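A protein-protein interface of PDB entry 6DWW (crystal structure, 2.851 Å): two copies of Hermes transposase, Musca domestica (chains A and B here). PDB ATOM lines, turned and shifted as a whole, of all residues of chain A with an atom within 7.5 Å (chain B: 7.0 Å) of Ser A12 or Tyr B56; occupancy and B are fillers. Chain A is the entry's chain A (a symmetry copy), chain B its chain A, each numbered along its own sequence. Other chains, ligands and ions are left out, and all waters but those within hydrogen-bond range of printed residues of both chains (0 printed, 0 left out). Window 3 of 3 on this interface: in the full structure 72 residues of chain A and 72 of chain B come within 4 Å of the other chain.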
ATOM      1  N   LYS A   9       3.840  19.822 -26.980  1.00  0.00           N
ATOM      2  CA  LYS A   9       2.422  20.136 -27.032  1.00  0.00           C
ATOM      3  C   LYS A   9       2.048  21.118 -25.930  1.00  0.00           C
ATOM      4  O   LYS A   9       2.539  21.030 -24.799  1.00  0.00           O
ATOM      5  CB  LYS A   9       1.589  18.861 -26.894  1.00  0.00           C
ATOM      6  CG  LYS A   9       2.342  17.587 -27.240  1.00  0.00           C
ATOM      7  CD  LYS A   9       1.543  16.345 -26.879  1.00  0.00           C
ATOM      8  CE  LYS A   9       2.404  15.090 -26.957  1.00  0.00           C
ATOM      9  NZ  LYS A   9       2.936  14.833 -28.324  1.00  0.00           N
ATOM     10  N   THR A  10       1.180  22.065 -26.274  1.00  0.00           N
ATOM     11  CA  THR A  10       0.587  22.966 -25.299  1.00  0.00           C
ATOM     12  C   THR A  10      -0.719  22.367 -24.795  1.00  0.00           C
ATOM     13  O   THR A  10      -1.508  21.827 -25.579  1.00  0.00           O
ATOM     14  CB  THR A  10       0.343  24.347 -25.916  1.00  0.00           C
ATOM     15  OG1 THR A  10       1.602  24.990 -26.159  1.00  0.00           O
ATOM     16  CG2 THR A  10      -0.500  25.213 -24.985  1.00  0.00           C
ATOM     17  N   VAL A  11      -0.933  22.442 -23.481  1.00  0.00           N
ATOM     18  CA  VAL A  11      -2.130  21.856 -22.901  1.00  0.00           C
ATOM     19  C   VAL A  11      -3.328  22.775 -23.118  1.00  0.00           C
ATOM     20  O   VAL A  11      -3.198  23.964 -23.432  1.00  0.00           O
ATOM     21  CB  VAL A  11      -1.925  21.555 -21.409  1.00  0.00           C
ATOM     22  CG1 VAL A  11      -0.865  20.483 -21.229  1.00  0.00           C
ATOM     23  CG2 VAL A  11      -1.542  22.819 -20.668  1.00  0.00           C
ATOM     24  N   SER A  12      -4.519  22.206 -22.949  1.00  0.00           N
ATOM     25  CA  SER A  12      -5.749  22.970 -23.087  1.00  0.00           C
ATOM     26  C   SER A  12      -5.862  24.004 -21.975  1.00  0.00           C
ATOM     27  O   SER A  12      -5.405  23.792 -20.848  1.00  0.00           O
ATOM     28  CB  SER A  12      -6.961  22.040 -23.061  1.00  0.00           C
ATOM     29  OG  SER A  12      -7.019  21.308 -21.849  1.00  0.00           O
ATOM     30  N   ALA A  13      -6.484  25.139 -22.304  1.00  0.00           N
ATOM     31  CA  ALA A  13      -6.656  26.200 -21.316  1.00  0.00           C
ATOM     32  C   ALA A  13      -7.496  25.735 -20.135  1.00  0.00           C
ATOM     33  O   ALA A  13      -7.332  26.240 -19.018  1.00  0.00           O
ATOM     34  CB  ALA A  13      -7.291  27.429 -21.965  1.00  0.00           C
ATOM     35  N   ASP A  14      -8.398  24.777 -20.361  1.00  0.00           N
ATOM     36  CA  ASP A  14      -9.146  24.195 -19.254  1.00  0.00           C
ATOM     37  C   ASP A  14      -8.247  23.351 -18.357  1.00  0.00           C
ATOM     38  O   ASP A  14      -8.542  23.180 -17.168  1.00  0.00           O
ATOM     39  CB  ASP A  14     -10.311  23.363 -19.795  1.00  0.00           C
ATOM     40  CG  ASP A  14     -11.295  24.193 -20.611  1.00  0.00           C
ATOM     41  OD1 ASP A  14     -11.843  23.672 -21.609  1.00  0.00           O
ATOM     42  OD2 ASP A  14     -11.520  25.368 -20.253  1.00  0.00           O
ATOM     43  N   CYS A  15      -7.150  22.821 -18.901  1.00  0.00           N
ATOM     44  CA  CYS A  15      -6.164  22.094 -18.112  1.00  0.00           C
ATOM     45  C   CYS A  15      -5.027  22.982 -17.625  1.00  0.00           C
ATOM     46  O   CYS A  15      -4.259  22.553 -16.757  1.00  0.00           O
ATOM     47  CB  CYS A  15      -5.585  20.925 -18.923  1.00  0.00           C
ATOM     48  SG  CYS A  15      -5.721  19.287 -18.138  1.00  0.00           S
ATOM     49  N   LYS A  16      -4.898  24.203 -18.153  1.00  0.00           N
ATOM     50  CA  LYS A  16      -3.826  25.098 -17.735  1.00  0.00           C
ATOM     51  C   LYS A  16      -4.245  26.007 -16.587  1.00  0.00           C
ATOM     52  O   LYS A  16      -3.426  26.316 -15.716  1.00  0.00           O
ATOM     53  CB  LYS A  16      -3.341  25.947 -18.914  1.00  0.00           C
ATOM     54  CG  LYS A  16      -2.020  26.655 -18.643  1.00  0.00           C
ATOM     55  CD  LYS A  16      -1.508  27.415 -19.858  1.00  0.00           C
ATOM     56  CE  LYS A  16      -1.966  28.868 -19.843  1.00  0.00           C
ATOM     57  NZ  LYS A  16      -1.374  29.648 -20.969  1.00  0.00           N
ATOM     58  N   LYS A  17      -5.505  26.454 -16.571  1.00  0.00           N
ATOM     59  CA  LYS A  17      -5.997  27.193 -15.414  1.00  0.00           C
ATOM     60  C   LYS A  17      -5.963  26.335 -14.157  1.00  0.00           C
ATOM     61  O   LYS A  17      -5.713  26.848 -13.062  1.00  0.00           O
ATOM     62  CB  LYS A  17      -7.417  27.704 -15.666  1.00  0.00           C
ATOM     63  CG  LYS A  17      -8.055  28.359 -14.441  1.00  0.00           C
ATOM     64  CD  LYS A  17      -7.195  29.511 -13.916  1.00  0.00           C
ATOM     65  CE  LYS A  17      -7.312  29.687 -12.398  1.00  0.00           C
ATOM     66  NZ  LYS A  17      -8.547  30.402 -11.964  1.00  0.00           N
ATOM     67  N   GLU A  18      -6.198  25.031 -14.290  1.00  0.00           N
ATOM     68  CA  GLU A  18      -6.115  24.153 -13.132  1.00  0.00           C
ATOM     69  C   GLU A  18      -4.685  23.997 -12.634  1.00  0.00           C
ATOM     70  O   GLU A  18      -4.482  23.676 -11.459  1.00  0.00           O
ATOM     71  CB  GLU A  18      -6.711  22.784 -13.465  1.00  0.00           C
ATOM     72  CG  GLU A  18      -7.118  21.966 -12.250  1.00  0.00           C
ATOM     73  CD  GLU A  18      -8.025  20.804 -12.612  1.00  0.00           C
ATOM     74  OE1 GLU A  18      -7.925  20.302 -13.754  1.00  0.00           O
ATOM     75  OE2 GLU A  18      -8.844  20.400 -11.760  1.00  0.00           O
ATOM     76  N   ILE A  50       5.777  14.349 -15.167  1.00  0.00           N
ATOM     77  CA  ILE A  50       4.846  14.087 -16.258  1.00  0.00           C
ATOM     78  C   ILE A  50       5.258  12.847 -17.041  1.00  0.00           C
ATOM     79  O   ILE A  50       4.409  12.221 -17.684  1.00  0.00           O
ATOM     80  CB  ILE A  50       4.701  15.296 -17.200  1.00  0.00           C
ATOM     81  CG1 ILE A  50       5.902  15.406 -18.138  1.00  0.00           C
ATOM     82  CG2 ILE A  50       4.519  16.583 -16.399  1.00  0.00           C
ATOM     83  CD1 ILE A  50       5.643  16.276 -19.348  1.00  0.00           C
ATOM     84  N   ALA A  54       2.959   9.412 -17.954  1.00  0.00           N
ATOM     85  CA  ALA A  54       2.846   8.836 -19.289  1.00  0.00           C
ATOM     86  C   ALA A  54       3.045   7.325 -19.250  1.00  0.00           C
ATOM     87  O   ALA A  54       2.244   6.571 -19.813  1.00  0.00           O
ATOM     88  CB  ALA A  54       3.854   9.493 -20.231  1.00  0.00           C
ATOM     89  N   LYS B  51      -1.179  13.418 -13.802  1.00  0.00           N
ATOM     90  CA  LYS B  51      -2.359  13.344 -14.657  1.00  0.00           C
ATOM     91  C   LYS B  51      -2.071  13.943 -16.026  1.00  0.00           C
ATOM     92  O   LYS B  51      -2.432  13.362 -17.055  1.00  0.00           O
ATOM     93  CB  LYS B  51      -3.542  14.053 -13.997  1.00  0.00           C
ATOM     94  CG  LYS B  51      -4.193  13.273 -12.866  1.00  0.00           C
ATOM     95  CD  LYS B  51      -5.251  14.106 -12.157  1.00  0.00           C
ATOM     96  CE  LYS B  51      -5.789  13.393 -10.924  1.00  0.00           C
ATOM     97  NZ  LYS B  51      -6.597  14.316 -10.075  1.00  0.00           N
ATOM     98  N   VAL B  52      -1.415  15.107 -16.056  1.00  0.00           N
ATOM     99  CA  VAL B  52      -1.100  15.763 -17.323  1.00  0.00           C
ATOM    100  C   VAL B  52      -0.213  14.877 -18.186  1.00  0.00           C
ATOM    101  O   VAL B  52      -0.319  14.892 -19.418  1.00  0.00           O
ATOM    102  CB  VAL B  52      -0.454  17.139 -17.059  1.00  0.00           C
ATOM    103  CG1 VAL B  52      -0.179  17.868 -18.368  1.00  0.00           C
ATOM    104  CG2 VAL B  52      -1.350  17.974 -16.166  1.00  0.00           C
ATOM    105  N   GLY B  53       0.658  14.082 -17.565  1.00  0.00           N
ATOM    106  CA  GLY B  53       1.465  13.145 -18.327  1.00  0.00           C
ATOM    107  C   GLY B  53       0.677  11.963 -18.853  1.00  0.00           C
ATOM    108  O   GLY B  53       1.048  11.368 -19.869  1.00  0.00           O
ATOM    109  N   ALA B  54      -0.413  11.601 -18.176  1.00  0.00           N
ATOM    110  CA  ALA B  54      -1.259  10.517 -18.662  1.00  0.00           C
ATOM    111  C   ALA B  54      -2.073  10.961 -19.871  1.00  0.00           C
ATOM    112  O   ALA B  54      -2.107  10.270 -20.895  1.00  0.00           O
ATOM    113  CB  ALA B  54      -2.173  10.021 -17.542  1.00  0.00           C
ATOM    114  N   GLU B  55      -2.730  12.117 -19.775  1.00  0.00           N
ATOM    115  CA  GLU B  55      -3.524  12.629 -20.887  1.00  0.00           C
ATOM    116  C   GLU B  55      -2.648  12.993 -22.078  1.00  0.00           C
ATOM    117  O   GLU B  55      -2.724  12.349 -23.129  1.00  0.00           O
ATOM    118  CB  GLU B  55      -4.343  13.851 -20.459  1.00  0.00           C
ATOM    119  CG  GLU B  55      -5.692  13.522 -19.843  1.00  0.00           C
ATOM    120  CD  GLU B  55      -5.632  13.402 -18.335  1.00  0.00           C
ATOM    121  OE1 GLU B  55      -5.485  14.445 -17.662  1.00  0.00           O
ATOM    122  OE2 GLU B  55      -5.724  12.266 -17.822  1.00  0.00           O
ATOM    123  N   TYR B  56      -1.806  14.017 -21.916  1.00  0.00           N
ATOM    124  CA  TYR B  56      -1.088  14.620 -23.031  1.00  0.00           C
ATOM    125  C   TYR B  56       0.195  13.889 -23.410  1.00  0.00           C
ATOM    126  O   TYR B  56       0.821  14.260 -24.408  1.00  0.00           O
ATOM    127  CB  TYR B  56      -0.753  16.080 -22.709  1.00  0.00           C
ATOM    128  CG  TYR B  56      -1.958  16.977 -22.511  1.00  0.00           C
ATOM    129  CD1 TYR B  56      -2.608  17.044 -21.284  1.00  0.00           C
ATOM    130  CD2 TYR B  56      -2.436  17.769 -23.547  1.00  0.00           C
ATOM    131  CE1 TYR B  56      -3.706  17.867 -21.098  1.00  0.00           C
ATOM    132  CE2 TYR B  56      -3.532  18.595 -23.372  1.00  0.00           C
ATOM    133  CZ  TYR B  56      -4.163  18.641 -22.146  1.00  0.00           C
ATOM    134  OH  TYR B  56      -5.253  19.463 -21.968  1.00  0.00           O
ATOM    135  N   GLY B  57       0.607  12.869 -22.659  1.00  0.00           N
ATOM    136  CA  GLY B  57       1.858  12.197 -22.945  1.00  0.00           C
ATOM    137  C   GLY B  57       3.037  12.923 -22.326  1.00  0.00           C
ATOM    138  O   GLY B  57       2.894  13.911 -21.607  1.00  0.00           O
ATOM    139  N   GLU B  58       4.235  12.429 -22.634  1.00  0.00           N
ATOM    140  CA  GLU B  58       5.439  12.895 -21.955  1.00  0.00           C
ATOM    141  C   GLU B  58       6.118  14.078 -22.642  1.00  0.00           C
ATOM    142  O   GLU B  58       7.135  14.565 -22.135  1.00  0.00           O
ATOM    143  CB  GLU B  58       6.439  11.739 -21.803  1.00  0.00           C
ATOM    144  CG  GLU B  58       7.454  11.597 -22.927  1.00  0.00           C
ATOM    145  CD  GLU B  58       8.625  10.709 -22.536  1.00  0.00           C
ATOM    146  OE1 GLU B  58       8.383   9.603 -22.006  1.00  0.00           O
ATOM    147  OE2 GLU B  58       9.788  11.124 -22.743  1.00  0.00           O
ATOM    148  N   HIS B  59       5.582  14.571 -23.758  1.00  0.00           N
ATOM    149  CA  HIS B  59       6.227  15.676 -24.460  1.00  0.00           C
ATOM    150  C   HIS B  59       5.417  16.964 -24.354  1.00  0.00           C
ATOM    151  O   HIS B  59       4.986  17.517 -25.371  1.00  0.00           O
ATOM    152  CB  HIS B  59       6.457  15.316 -25.932  1.00  0.00           C
ATOM    153  CG  HIS B  59       7.459  14.221 -26.138  1.00  0.00           C
ATOM    154  ND1 HIS B  59       8.728  14.261 -25.600  1.00  0.00           N
ATOM    155  CD2 HIS B  59       7.382  13.061 -26.831  1.00  0.00           C
ATOM    156  CE1 HIS B  59       9.386  13.170 -25.946  1.00  0.00           C
ATOM    157  NE2 HIS B  59       8.592  12.425 -26.694  1.00  0.00           N
ATOM    158  N   VAL B  60       5.223  17.458 -23.135  1.00  0.00           N
ATOM    159  CA  VAL B  60       4.439  18.663 -22.893  1.00  0.00           C
ATOM    160  C   VAL B  60       5.375  19.849 -22.698  1.00  0.00           C
ATOM    161  O   VAL B  60       6.468  19.723 -22.130  1.00  0.00           O
ATOM    162  CB  VAL B  60       3.509  18.478 -21.675  1.00  0.00           C
ATOM    163  CG1 VAL B  60       2.588  19.677 -21.513  1.00  0.00           C
ATOM    164  CG2 VAL B  60       2.706  17.193 -21.810  1.00  0.00           C
ATOM    165  N   LEU B  65       3.217  25.619 -19.615  1.00  0.00           N
ATOM    166  CA  LEU B  65       2.204  25.085 -18.707  1.00  0.00           C
ATOM    167  C   LEU B  65       2.333  25.692 -17.313  1.00  0.00           C
ATOM    168  O   LEU B  65       1.322  26.002 -16.668  1.00  0.00           O
ATOM    169  CB  LEU B  65       2.328  23.560 -18.650  1.00  0.00           C
ATOM    170  CG  LEU B  65       1.274  22.625 -18.034  1.00  0.00           C
ATOM    171  CD1 LEU B  65       1.899  21.795 -16.920  1.00  0.00           C
ATOM    172  CD2 LEU B  65       0.008  23.333 -17.547  1.00  0.00           C
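The backbone carbonyl oxygen (O) of Gly B53 sits close to the backbone NH (N) of Ala A54.
The side-chain hydroxyl (OH) of Tyr B56 sits at hydrogen-bond distance from the side-chain hydroxyl (OG) of Ser A12 (2.6 Å).
O of His B59 sits at hydrogen-bond distance from N of Lys A9, 3.0 Å away.
OG of Ser A12 lies close to N of Cys A15 (3.3 Å).
Among the printed residues, merely in contact across the chains: Lys A9 with Tyr B56, Lys A9 with Val B60, Val A11 with Val B52, Val A11 with Tyr B56, Val A11 with Val B60, Val A11 with Leu B65, Cys A15 with Tyr B56, Lys A16 with Leu B65, Ile A50 with Gly B53, Ile A50 with Glu B58, Ile A50 with Val B60 and Ala A54 with Glu B58.
Of chain B, only Tyr B56 (2.6 Å) comes within 4 Å of Ser A12.
Of chain A, only Lys A9 (3.1 Å), Val A11 (3.6 Å), Ser A12 (2.6 Å) and Cys A15 (3.4 Å) come within 4 Å of Tyr B56.
No residue of chain A comes within 4 Å of Gly B57.
Of the printed residues of chain B, Val A11 touches Val B52 (3.9 Å), Tyr B56 (3.6 Å), Val B60 (3.6 Å) and Leu B65 (3.5 Å).
Printed residues of chain A within 4 Å of Val B60: Lys A9, Val A11 and Ile A50.
Of the printed residues of chain B, Lys A16 touches Leu B65 (3.9 Å).
Thr A10 touches none of the printed residues of chain B.
Lys B51 touches none of the printed residues of chain A.
The nearest residue of chain B that does not touch Ser A12 is Leu B65 (6.4 Å).
Hydrophobic or aromatic side chains of chain B that line the printed part of chain A: Val B52, Tyr B56, Val B60 and Leu B65.
Printed residues of chain A that touch a printed residue of chain B: Lys A9, Val A11, Ser A12, Cys A15, Lys A16, Ile A50 and Ala A54.
Hydrophobic or aromatic side chains of chain A within 4 Å of the printed part of chain B: Val A11, Ile A50 and Ala A54.
Among the printed residues, no Asp or Glu carboxylate lies within 4 Å of a Lys or Arg side-chain nitrogen of the other chain.
Position printed for both chains: 54.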
